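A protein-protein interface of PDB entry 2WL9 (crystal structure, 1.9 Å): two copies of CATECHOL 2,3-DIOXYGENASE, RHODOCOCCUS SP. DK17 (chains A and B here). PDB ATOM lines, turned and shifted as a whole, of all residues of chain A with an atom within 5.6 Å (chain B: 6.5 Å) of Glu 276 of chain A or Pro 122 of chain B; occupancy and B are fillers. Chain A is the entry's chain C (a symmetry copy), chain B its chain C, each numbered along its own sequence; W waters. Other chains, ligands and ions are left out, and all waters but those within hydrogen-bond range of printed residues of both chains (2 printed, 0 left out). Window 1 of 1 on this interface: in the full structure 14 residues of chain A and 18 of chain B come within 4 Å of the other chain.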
ATOM      1  N   VAL A 173     -15.705 -14.187 -29.849  1.00  0.00           N
ATOM      2  CA  VAL A 173     -15.660 -12.800 -30.301  1.00  0.00           C
ATOM      3  C   VAL A 173     -16.469 -11.903 -29.363  1.00  0.00           C
ATOM      4  O   VAL A 173     -17.589 -12.241 -28.996  1.00  0.00           O
ATOM      5  CB  VAL A 173     -16.215 -12.688 -31.733  1.00  0.00           C
ATOM      6  CG1 VAL A 173     -16.356 -11.224 -32.142  1.00  0.00           C
ATOM      7  CG2 VAL A 173     -15.321 -13.449 -32.708  1.00  0.00           C
ATOM      8  N   GLU A 174     -15.902 -10.767 -28.965  1.00  0.00           N
ATOM      9  CA  GLU A 174     -16.647  -9.843 -28.111  1.00  0.00           C
ATOM     10  C   GLU A 174     -16.882  -8.477 -28.732  1.00  0.00           C
ATOM     11  O   GLU A 174     -17.693  -7.704 -28.243  1.00  0.00           O
ATOM     12  CB  GLU A 174     -16.001  -9.721 -26.730  1.00  0.00           C
ATOM     13  CG  GLU A 174     -16.233 -10.945 -25.866  1.00  0.00           C
ATOM     14  CD  GLU A 174     -15.827 -10.747 -24.421  1.00  0.00           C
ATOM     15  OE1 GLU A 174     -15.085  -9.791 -24.133  1.00  0.00           O
ATOM     16  OE2 GLU A 174     -16.238 -11.560 -23.574  1.00  0.00           O
ATOM     17  N   ARG A 269     -15.327  -6.045 -14.048  1.00  0.00           N
ATOM     18  CA  ARG A 269     -16.457  -6.915 -13.714  1.00  0.00           C
ATOM     19  C   ARG A 269     -16.151  -8.362 -14.105  1.00  0.00           C
ATOM     20  O   ARG A 269     -15.283  -8.607 -14.952  1.00  0.00           O
ATOM     21  CB  ARG A 269     -17.745  -6.437 -14.399  1.00  0.00           C
ATOM     22  CG  ARG A 269     -17.846  -6.789 -15.879  1.00  0.00           C
ATOM     23  CD  ARG A 269     -19.231  -6.453 -16.429  1.00  0.00           C
ATOM     24  NE  ARG A 269     -19.335  -6.785 -17.848  1.00  0.00           N
ATOM     25  CZ  ARG A 269     -20.469  -7.115 -18.464  1.00  0.00           C
ATOM     26  NH1 ARG A 269     -21.610  -7.171 -17.787  1.00  0.00           N
ATOM     27  NH2 ARG A 269     -20.457  -7.405 -19.759  1.00  0.00           N
ATOM     28  N   PRO A 272     -19.459 -12.294 -18.132  1.00  0.00           N
ATOM     29  CA  PRO A 272     -20.863 -12.712 -18.130  1.00  0.00           C
ATOM     30  C   PRO A 272     -20.954 -14.222 -18.303  1.00  0.00           C
ATOM     31  O   PRO A 272     -20.109 -14.815 -18.984  1.00  0.00           O
ATOM     32  CB  PRO A 272     -21.448 -12.009 -19.358  1.00  0.00           C
ATOM     33  CG  PRO A 272     -20.504 -10.886 -19.656  1.00  0.00           C
ATOM     34  CD  PRO A 272     -19.158 -11.399 -19.264  1.00  0.00           C
ATOM     35  N   GLN A 274     -22.910 -15.853 -20.007  1.00  0.00           N
ATOM     36  CA  GLN A 274     -23.208 -16.170 -21.399  1.00  0.00           C
ATOM     37  C   GLN A 274     -22.612 -15.135 -22.343  1.00  0.00           C
ATOM     38  O   GLN A 274     -22.528 -13.959 -22.005  1.00  0.00           O
ATOM     39  CB  GLN A 274     -24.710 -16.246 -21.604  1.00  0.00           C
ATOM     40  CG  GLN A 274     -25.413 -17.118 -20.588  1.00  0.00           C
ATOM     41  CD  GLN A 274     -26.864 -17.269 -20.899  1.00  0.00           C
ATOM     42  OE1 GLN A 274     -27.723 -17.066 -20.039  1.00  0.00           O
ATOM     43  NE2 GLN A 274     -27.161 -17.620 -22.146  1.00  0.00           N
ATOM     44  N   GLN A 275     -22.214 -15.596 -23.526  1.00  0.00           N
ATOM     45  CA  GLN A 275     -21.468 -14.793 -24.491  1.00  0.00           C
ATOM     46  C   GLN A 275     -22.249 -13.566 -24.953  1.00  0.00           C
ATOM     47  O   GLN A 275     -23.430 -13.661 -25.262  1.00  0.00           O
ATOM     48  CB  GLN A 275     -21.081 -15.665 -25.689  1.00  0.00           C
ATOM     49  CG  GLN A 275     -20.049 -15.074 -26.628  1.00  0.00           C
ATOM     50  CD  GLN A 275     -18.737 -14.759 -25.940  1.00  0.00           C
ATOM     51  OE1 GLN A 275     -18.237 -15.531 -25.107  1.00  0.00           O
ATOM     52  NE2 GLN A 275     -18.168 -13.613 -26.288  1.00  0.00           N
ATOM     53  N   GLU A 276     -21.561 -12.422 -24.984  1.00  0.00           N
ATOM     54  CA  GLU A 276     -22.122 -11.141 -25.431  1.00  0.00           C
ATOM     55  C   GLU A 276     -21.148 -10.514 -26.423  1.00  0.00           C
ATOM     56  O   GLU A 276     -19.957 -10.822 -26.400  1.00  0.00           O
ATOM     57  CB  GLU A 276     -22.274 -10.176 -24.244  1.00  0.00           C
ATOM     58  CG  GLU A 276     -23.422 -10.457 -23.277  1.00  0.00           C
ATOM     59  CD  GLU A 276     -23.443  -9.512 -22.069  1.00  0.00           C
ATOM     60  OE1 GLU A 276     -22.712  -8.497 -22.054  1.00  0.00           O
ATOM     61  OE2 GLU A 276     -24.214  -9.777 -21.128  1.00  0.00           O
ATOM     62  N   HIS A 277     -21.635  -9.621 -27.280  1.00  0.00           N
ATOM     63  CA  HIS A 277     -20.719  -8.819 -28.096  1.00  0.00           C
ATOM     64  C   HIS A 277     -21.134  -7.347 -28.182  1.00  0.00           C
ATOM     65  O   HIS A 277     -22.274  -6.992 -27.874  1.00  0.00           O
ATOM     66  CB  HIS A 277     -20.459  -9.449 -29.484  1.00  0.00           C
ATOM     67  CG  HIS A 277     -21.504  -9.135 -30.512  1.00  0.00           C
ATOM     68  ND1 HIS A 277     -22.642  -9.895 -30.675  1.00  0.00           N
ATOM     69  CD2 HIS A 277     -21.567  -8.160 -31.448  1.00  0.00           C
ATOM     70  CE1 HIS A 277     -23.367  -9.396 -31.660  1.00  0.00           C
ATOM     71  NE2 HIS A 277     -22.741  -8.337 -32.141  1.00  0.00           N
ATOM     72  N   TYR A 278     -20.187  -6.500 -28.586  1.00  0.00           N
ATOM     73  CA  TYR A 278     -20.363  -5.052 -28.541  1.00  0.00           C
ATOM     74  C   TYR A 278     -19.857  -4.423 -29.829  1.00  0.00           C
ATOM     75  O   TYR A 278     -19.103  -5.051 -30.574  1.00  0.00           O
ATOM     76  CB  TYR A 278     -19.622  -4.476 -27.326  1.00  0.00           C
ATOM     77  CG  TYR A 278     -19.806  -5.322 -26.083  1.00  0.00           C
ATOM     78  CD1 TYR A 278     -18.863  -6.279 -25.721  1.00  0.00           C
ATOM     79  CD2 TYR A 278     -20.945  -5.187 -25.286  1.00  0.00           C
ATOM     80  CE1 TYR A 278     -19.042  -7.081 -24.598  1.00  0.00           C
ATOM     81  CE2 TYR A 278     -21.126  -5.980 -24.146  1.00  0.00           C
ATOM     82  CZ  TYR A 278     -20.166  -6.924 -23.813  1.00  0.00           C
ATOM     83  OH  TYR A 278     -20.335  -7.716 -22.699  1.00  0.00           O
ATOM     84  N   ARG B  47     -30.250  -3.646 -21.767  1.00  0.00           N
ATOM     85  CA  ARG B  47     -28.922  -3.414 -22.353  1.00  0.00           C
ATOM     86  C   ARG B  47     -28.774  -3.884 -23.811  1.00  0.00           C
ATOM     87  O   ARG B  47     -28.058  -3.259 -24.598  1.00  0.00           O
ATOM     88  CB  ARG B  47     -27.871  -4.140 -21.523  1.00  0.00           C
ATOM     89  CG  ARG B  47     -27.138  -3.336 -20.461  1.00  0.00           C
ATOM     90  CD  ARG B  47     -25.851  -4.103 -20.076  1.00  0.00           C
ATOM     91  NE  ARG B  47     -26.094  -5.546 -20.129  1.00  0.00           N
ATOM     92  CZ  ARG B  47     -25.177  -6.488 -20.353  1.00  0.00           C
ATOM     93  NH1 ARG B  47     -23.892  -6.187 -20.534  1.00  0.00           N
ATOM     94  NH2 ARG B  47     -25.559  -7.753 -20.388  1.00  0.00           N
ATOM     95  N   TRP B  48     -29.410  -5.008 -24.146  1.00  0.00           N
ATOM     96  CA  TRP B  48     -29.336  -5.588 -25.492  1.00  0.00           C
ATOM     97  C   TRP B  48     -29.796  -4.585 -26.535  1.00  0.00           C
ATOM     98  O   TRP B  48     -30.721  -3.809 -26.290  1.00  0.00           O
ATOM     99  CB  TRP B  48     -30.238  -6.818 -25.611  1.00  0.00           C
ATOM    100  CG  TRP B  48     -29.810  -8.047 -24.859  1.00  0.00           C
ATOM    101  CD1 TRP B  48     -29.116  -8.108 -23.670  1.00  0.00           C
ATOM    102  CD2 TRP B  48     -30.120  -9.400 -25.213  1.00  0.00           C
ATOM    103  NE1 TRP B  48     -28.938  -9.424 -23.297  1.00  0.00           N
ATOM    104  CE2 TRP B  48     -29.550 -10.234 -24.222  1.00  0.00           C
ATOM    105  CE3 TRP B  48     -30.802  -9.991 -26.291  1.00  0.00           C
ATOM    106  CZ2 TRP B  48     -29.657 -11.636 -24.269  1.00  0.00           C
ATOM    107  CZ3 TRP B  48     -30.905 -11.382 -26.341  1.00  0.00           C
ATOM    108  CH2 TRP B  48     -30.333 -12.189 -25.335  1.00  0.00           C
ATOM    109  N   HIS B  49     -29.156  -4.607 -27.702  1.00  0.00           N
ATOM    110  CA  HIS B  49     -29.596  -3.787 -28.826  1.00  0.00           C
ATOM    111  C   HIS B  49     -31.121  -3.861 -28.961  1.00  0.00           C
ATOM    112  O   HIS B  49     -31.786  -2.825 -29.111  1.00  0.00           O
ATOM    113  CB  HIS B  49     -28.919  -4.243 -30.121  1.00  0.00           C
ATOM    114  CG  HIS B  49     -29.448  -3.562 -31.344  1.00  0.00           C
ATOM    115  ND1 HIS B  49     -30.417  -4.126 -32.147  1.00  0.00           N
ATOM    116  CD2 HIS B  49     -29.156  -2.360 -31.894  1.00  0.00           C
ATOM    117  CE1 HIS B  49     -30.696  -3.305 -33.142  1.00  0.00           C
ATOM    118  NE2 HIS B  49     -29.939  -2.229 -33.017  1.00  0.00           N
ATOM    119  N   HIS B  50     -31.669  -5.076 -28.868  1.00  0.00           N
ATOM    120  CA  HIS B  50     -33.121  -5.282 -28.958  1.00  0.00           C
ATOM    121  C   HIS B  50     -33.579  -6.620 -28.378  1.00  0.00           C
ATOM    122  O   HIS B  50     -32.790  -7.570 -28.280  1.00  0.00           O
ATOM    123  CB  HIS B  50     -33.589  -5.202 -30.419  1.00  0.00           C
ATOM    124  CG  HIS B  50     -33.144  -6.365 -31.251  1.00  0.00           C
ATOM    125  ND1 HIS B  50     -31.901  -6.425 -31.836  1.00  0.00           N
ATOM    126  CD2 HIS B  50     -33.769  -7.521 -31.575  1.00  0.00           C
ATOM    127  CE1 HIS B  50     -31.778  -7.565 -32.490  1.00  0.00           C
ATOM    128  NE2 HIS B  50     -32.895  -8.251 -32.343  1.00  0.00           N
ATOM    129  N   ARG B  68     -31.616 -18.451 -26.679  1.00  0.00           N
ATOM    130  CA  ARG B  68     -30.193 -18.235 -26.435  1.00  0.00           C
ATOM    131  C   ARG B  68     -29.463 -19.439 -25.832  1.00  0.00           C
ATOM    132  O   ARG B  68     -30.003 -20.150 -24.979  1.00  0.00           O
ATOM    133  CB  ARG B  68     -30.011 -17.018 -25.524  1.00  0.00           C
ATOM    134  CG  ARG B  68     -28.577 -16.529 -25.386  1.00  0.00           C
ATOM    135  CD  ARG B  68     -28.470 -15.572 -24.205  1.00  0.00           C
ATOM    136  NE  ARG B  68     -27.193 -14.861 -24.182  1.00  0.00           N
ATOM    137  CZ  ARG B  68     -26.833 -13.996 -23.238  1.00  0.00           C
ATOM    138  NH1 ARG B  68     -27.654 -13.733 -22.227  1.00  0.00           N
ATOM    139  NH2 ARG B  68     -25.651 -13.390 -23.303  1.00  0.00           N
ATOM    140  N   VAL B  69     -28.229 -19.655 -26.279  1.00  0.00           N
ATOM    141  CA  VAL B  69     -27.308 -20.561 -25.603  1.00  0.00           C
ATOM    142  C   VAL B  69     -26.082 -19.759 -25.182  1.00  0.00           C
ATOM    143  O   VAL B  69     -25.884 -18.635 -25.646  1.00  0.00           O
ATOM    144  CB  VAL B  69     -26.923 -21.800 -26.458  1.00  0.00           C
ATOM    145  CG1 VAL B  69     -28.135 -22.679 -26.712  1.00  0.00           C
ATOM    146  CG2 VAL B  69     -26.265 -21.403 -27.769  1.00  0.00           C
ATOM    147  N   ALA B  70     -25.279 -20.327 -24.290  1.00  0.00           N
ATOM    148  CA  ALA B  70     -24.168 -19.601 -23.676  1.00  0.00           C
ATOM    149  C   ALA B  70     -23.033 -19.231 -24.633  1.00  0.00           C
ATOM    150  O   ALA B  70     -22.378 -18.206 -24.441  1.00  0.00           O
ATOM    151  CB  ALA B  70     -23.614 -20.391 -22.484  1.00  0.00           C
ATOM    152  N   ARG B 100     -29.602 -10.772 -37.426  1.00  0.00           N
ATOM    153  CA  ARG B 100     -30.251 -10.960 -36.123  1.00  0.00           C
ATOM    154  C   ARG B 100     -29.530 -10.237 -34.974  1.00  0.00           C
ATOM    155  O   ARG B 100     -30.019 -10.224 -33.837  1.00  0.00           O
ATOM    156  CB  ARG B 100     -30.353 -12.460 -35.805  1.00  0.00           C
ATOM    157  CG  ARG B 100     -31.210 -13.270 -36.784  1.00  0.00           C
ATOM    158  CD  ARG B 100     -32.703 -12.948 -36.669  1.00  0.00           C
ATOM    159  NE  ARG B 100     -33.483 -13.908 -37.448  1.00  0.00           N
ATOM    160  CZ  ARG B 100     -33.990 -13.682 -38.659  1.00  0.00           C
ATOM    161  NH1 ARG B 100     -33.851 -12.499 -39.251  1.00  0.00           N
ATOM    162  NH2 ARG B 100     -34.664 -14.643 -39.271  1.00  0.00           N
ATOM    163  N   ARG B 101     -28.388  -9.626 -35.283  1.00  0.00           N
ATOM    164  CA  ARG B 101     -27.473  -8.998 -34.296  1.00  0.00           C
ATOM    165  C   ARG B 101     -26.959  -9.999 -33.258  1.00  0.00           C
ATOM    166  O   ARG B 101     -27.018  -9.754 -32.044  1.00  0.00           O
ATOM    167  CB  ARG B 101     -28.088  -7.767 -33.601  1.00  0.00           C
ATOM    168  CG  ARG B 101     -28.839  -6.804 -34.491  1.00  0.00           C
ATOM    169  CD  ARG B 101     -27.972  -6.254 -35.609  1.00  0.00           C
ATOM    170  NE  ARG B 101     -28.719  -5.250 -36.353  1.00  0.00           N
ATOM    171  CZ  ARG B 101     -28.739  -3.960 -36.041  1.00  0.00           C
ATOM    172  NH1 ARG B 101     -28.036  -3.506 -35.006  1.00  0.00           N
ATOM    173  NH2 ARG B 101     -29.469  -3.120 -36.768  1.00  0.00           N
ATOM    174  N   VAL B 102     -26.456 -11.125 -33.752  1.00  0.00           N
ATOM    175  CA  VAL B 102     -25.889 -12.183 -32.914  1.00  0.00           C
ATOM    176  C   VAL B 102     -24.563 -12.650 -33.513  1.00  0.00           C
ATOM    177  O   VAL B 102     -24.205 -12.259 -34.632  1.00  0.00           O
ATOM    178  CB  VAL B 102     -26.851 -13.399 -32.747  1.00  0.00           C
ATOM    179  CG1 VAL B 102     -28.146 -12.979 -32.063  1.00  0.00           C
ATOM    180  CG2 VAL B 102     -27.127 -14.097 -34.098  1.00  0.00           C
ATOM    181  N   LEU B 103     -23.837 -13.478 -32.771  1.00  0.00           N
ATOM    182  CA  LEU B 103     -22.562 -13.993 -33.259  1.00  0.00           C
ATOM    183  C   LEU B 103     -22.674 -15.284 -34.059  1.00  0.00           C
ATOM    184  O   LEU B 103     -21.922 -15.492 -35.015  1.00  0.00           O
ATOM    185  CB  LEU B 103     -21.592 -14.206 -32.105  1.00  0.00           C
ATOM    186  CG  LEU B 103     -21.052 -12.980 -31.376  1.00  0.00           C
ATOM    187  CD1 LEU B 103     -20.132 -13.468 -30.269  1.00  0.00           C
ATOM    188  CD2 LEU B 103     -20.312 -12.029 -32.324  1.00  0.00           C
ATOM    189  N   PHE B 119     -29.233 -19.302 -30.863  1.00  0.00           N
ATOM    190  CA  PHE B 119     -28.154 -18.352 -31.085  1.00  0.00           C
ATOM    191  C   PHE B 119     -27.323 -18.122 -29.833  1.00  0.00           C
ATOM    192  O   PHE B 119     -27.766 -18.432 -28.719  1.00  0.00           O
ATOM    193  CB  PHE B 119     -28.749 -17.007 -31.526  1.00  0.00           C
ATOM    194  CG  PHE B 119     -29.362 -16.214 -30.395  1.00  0.00           C
ATOM    195  CD1 PHE B 119     -28.624 -15.237 -29.733  1.00  0.00           C
ATOM    196  CD2 PHE B 119     -30.674 -16.446 -29.998  1.00  0.00           C
ATOM    197  CE1 PHE B 119     -29.192 -14.487 -28.690  1.00  0.00           C
ATOM    198  CE2 PHE B 119     -31.256 -15.710 -28.952  1.00  0.00           C
ATOM    199  CZ  PHE B 119     -30.512 -14.722 -28.299  1.00  0.00           C
ATOM    200  N   TYR B 120     -26.142 -17.545 -30.025  1.00  0.00           N
ATOM    201  CA  TYR B 120     -25.305 -17.044 -28.926  1.00  0.00           C
ATOM    202  C   TYR B 120     -24.733 -15.671 -29.293  1.00  0.00           C
ATOM    203  O   TYR B 120     -24.663 -15.314 -30.471  1.00  0.00           O
ATOM    204  CB  TYR B 120     -24.149 -18.020 -28.607  1.00  0.00           C
ATOM    205  CG  TYR B 120     -23.036 -18.022 -29.642  1.00  0.00           C
ATOM    206  CD1 TYR B 120     -21.948 -17.145 -29.530  1.00  0.00           C
ATOM    207  CD2 TYR B 120     -23.078 -18.884 -30.741  1.00  0.00           C
ATOM    208  CE1 TYR B 120     -20.940 -17.130 -30.481  1.00  0.00           C
ATOM    209  CE2 TYR B 120     -22.071 -18.877 -31.698  1.00  0.00           C
ATOM    210  CZ  TYR B 120     -21.008 -17.993 -31.563  1.00  0.00           C
ATOM    211  OH  TYR B 120     -20.014 -17.984 -32.503  1.00  0.00           O
ATOM    212  N   GLY B 121     -24.308 -14.919 -28.279  1.00  0.00           N
ATOM    213  CA  GLY B 121     -23.651 -13.627 -28.486  1.00  0.00           C
ATOM    214  C   GLY B 121     -24.555 -12.510 -28.987  1.00  0.00           C
ATOM    215  O   GLY B 121     -24.343 -11.987 -30.091  1.00  0.00           O
ATOM    216  N   PRO B 122     -25.558 -12.113 -28.181  1.00  0.00           N
ATOM    217  CA  PRO B 122     -26.361 -10.953 -28.572  1.00  0.00           C
ATOM    218  C   PRO B 122     -25.517  -9.689 -28.584  1.00  0.00           C
ATOM    219  O   PRO B 122     -24.571  -9.570 -27.788  1.00  0.00           O
ATOM    220  CB  PRO B 122     -27.393 -10.848 -27.449  1.00  0.00           C
ATOM    221  CG  PRO B 122     -26.716 -11.475 -26.269  1.00  0.00           C
ATOM    222  CD  PRO B 122     -25.965 -12.631 -26.859  1.00  0.00           C
ATOM    223  N   GLN B 123     -25.848  -8.770 -29.492  1.00  0.00           N
ATOM    224  CA  GLN B 123     -25.283  -7.430 -29.491  1.00  0.00           C
ATOM    225  C   GLN B 123     -25.854  -6.655 -28.301  1.00  0.00           C
ATOM    226  O   GLN B 123     -27.068  -6.526 -28.155  1.00  0.00           O
ATOM    227  CB  GLN B 123     -25.605  -6.700 -30.808  1.00  0.00           C
ATOM    228  CG  GLN B 123     -25.132  -5.235 -30.872  1.00  0.00           C
ATOM    229  CD  GLN B 123     -25.671  -4.479 -32.086  1.00  0.00           C
ATOM    230  OE1 GLN B 123     -25.916  -5.059 -33.145  1.00  0.00           O
ATOM    231  NE2 GLN B 123     -25.858  -3.177 -31.930  1.00  0.00           N
ATOM    232  N   VAL B 124     -24.960  -6.147 -27.464  1.00  0.00           N
ATOM    233  CA  VAL B 124     -25.332  -5.366 -26.291  1.00  0.00           C
ATOM    234  C   VAL B 124     -24.841  -3.932 -26.496  1.00  0.00           C
ATOM    235  O   VAL B 124     -23.674  -3.700 -26.853  1.00  0.00           O
ATOM    236  CB  VAL B 124     -24.737  -6.005 -24.999  1.00  0.00           C
ATOM    237  CG1 VAL B 124     -25.184  -5.260 -23.741  1.00  0.00           C
ATOM    238  CG2 VAL B 124     -25.140  -7.470 -24.905  1.00  0.00           C
ATOM    239  N   THR B 126     -24.208  -1.348 -24.462  1.00  0.00           N
ATOM    240  CA  THR B 126     -23.907  -0.856 -23.127  1.00  0.00           C
ATOM    241  C   THR B 126     -23.728   0.660 -23.145  1.00  0.00           C
ATOM    242  O   THR B 126     -24.184   1.347 -22.226  1.00  0.00           O
ATOM    243  CB  THR B 126     -22.666  -1.577 -22.540  1.00  0.00           C
ATOM    244  OG1 THR B 126     -22.848  -2.992 -22.661  1.00  0.00           O
ATOM    245  CG2 THR B 126     -22.460  -1.233 -21.056  1.00  0.00           C
ATOM    246  N   GLU B 143     -32.758  -9.912 -17.183  1.00  0.00           N
ATOM    247  CA  GLU B 143     -31.413 -10.427 -16.940  1.00  0.00           C
ATOM    248  C   GLU B 143     -31.392 -11.899 -16.530  1.00  0.00           C
ATOM    249  O   GLU B 143     -31.820 -12.259 -15.434  1.00  0.00           O
ATOM    250  CB  GLU B 143     -30.707  -9.567 -15.882  1.00  0.00           C
ATOM    251  CG  GLU B 143     -29.235  -9.905 -15.673  1.00  0.00           C
ATOM    252  CD  GLU B 143     -28.369  -9.537 -16.860  1.00  0.00           C
ATOM    253  OE1 GLU B 143     -28.344  -8.339 -17.232  1.00  0.00           O
ATOM    254  OE2 GLU B 143     -27.707 -10.449 -17.417  1.00  0.00           O
HETATM  255  O   HOH W   1     -25.060 -16.048 -25.675  1.00  0.00           O
HETATM  256  O   HOH W   2     -21.592  -4.591 -20.933  1.00  0.00           O
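No position is printed for both chains. Of the 23 pairs that touch across the chains among the printed residues, none has its exchanged pair printed and touching as well.
Printed residues of chain B within 4 Å of Gln 274 of chain A: Arg 68 (3.2 Å), Val 69 (3.9 Å) and Ala 70 (3.7 Å). Glu 276 of chain A touches just these residues of chain B: Arg 47 (2.5 Å), Arg 68 (3.7 Å), Pro 122 (3.7 Å) and Val 124 (3.8 Å). His 50 of chain B touches none of the printed residues of chain A. Printed residues of chain A within 4 Å of Val 69 of chain B: Gln 274 (3.9 Å). Arg 100 of chain B touches none of the printed residues of chain A. Printed residues of chain A within 4 Å of Val 102 of chain B: His 277. Of chain A, only Gln 275 (3.2 Å), Glu 276 (3.7 Å) and His 277 (3.0 Å) come within 4 Å of Pro 122 of chain B.
Water W2 lies within hydrogen-bond range of OG1 of Thr 126 of chain B, NH1 of Arg 47 of chain B and NH2 of Arg 269 of chain A. Water W1 lies within hydrogen-bond range of O of Val 69 of chain B (2.7 Å), NE of Arg 68 of chain B (2.9 Å), O of Gln 275 of chain A (2.9 Å) and N of Gly 121 of chain B (2.9 Å).
The backbone carbonyl oxygen (O) of Gln 123 of chain B sits at hydrogen-bond distance from the backbone NH (N) of His 49 of chain B, at 2.9 Å. O of Phe 119 of chain B sits at hydrogen-bond distance from N of Val 69 of chain B, 2.8 Å away. The backbone NH (N) of Gln 123 of chain B is in hydrogen-bond range of the backbone carbonyl oxygen (O) of Arg 101 of chain B (3.0 Å). The backbone carbonyl oxygen (O) of Val 173 of chain A sits at hydrogen-bond distance from the side-chain amide nitrogen (NE2) of Gln 275 of chain A (3.1 Å). NH2 of Arg 269 of chain A is in salt-bridge range of OE1 of Glu 276 of chain A. The guanidinium group (NH2) of Arg 269 of chain A lies within hydrogen-bond range of the side-chain hydroxyl (OH) of Tyr 278 of chain A (3.0 Å).
Leu 103 of chain B touches Val 173 of chain A. Gln 274 of chain A touches Val 69 of chain B (NE2 to O, 3.9 Å). Gln 274 of chain A touches Ala 70 of chain B (C to O, 3.7 Å). Gln 275 of chain A touches Leu 103 of chain B (CG to CD1, 3.98 Å). Glu 276 of chain A touches Arg 68 of chain B (CG to NH2, 3.7 Å). Glu 276 of chain A touches Pro 122 of chain B (CA to O, 3.7 Å). His 277 of chain A touches Val 102 of chain B (CE1 to C, 3.9 Å). His 277 of chain A touches Leu 103 of chain B. Gln 123 of chain B touches His 277 of chain A. CE2 of Tyr 278 of chain A touches OG1 of Thr 126 of chain B (3.8 Å).
OE2 of Glu 276 of chain A is in salt-bridge range of NH2 of Arg 47 of chain B. The guanidinium group (NE) of Arg 68 of chain B sits close to the side-chain amide nitrogen (NE2) of Gln 274 of chain A (3.4 Å). NH2 of Arg 68 of chain B lies within hydrogen-bond range of O of Gln 275 of chain A (3.0 Å). The backbone carbonyl oxygen of Ala 70 of chain B sits at hydrogen-bond distance from the backbone NH of Gln 275 of chain A (2.8 Å). The backbone carbonyl oxygen (O) of Gln 275 of chain A lies close to the backbone NH (N) of Gly 121 of chain B (3.4 Å). O of Gly 121 of chain B sits at hydrogen-bond distance from ND1 of His 277 of chain A, at 2.8 Å. O of Pro 122 of chain B is in hydrogen-bond range of N of His 277 of chain A (3.0 Å). O of His 277 of chain A lies within hydrogen-bond range of N of Val 124 of chain B (2.8 Å).
Hydrophobic or aromatic side chains of chain A within 4 Å of the printed part of chain B: His 277 and Tyr 278. Of the 19 printed residues of chain B, 12 touch a printed residue of chain A. Printed residues of chain B that touch a printed residue of chain A: Arg 47, Arg 68, Val 69, Ala 70, Arg 101, Val 102, Leu 103, Gly 121, Pro 122, Gln 123, Val 124 and Thr 126. Among the printed residues, 23 pairs touch across the chains. Among the printed residues, Asp or Glu carboxylates within 4 Å of a Lys or Arg side-chain nitrogen of the other chain: Glu 276 of chain A with Arg 47 of chain B.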
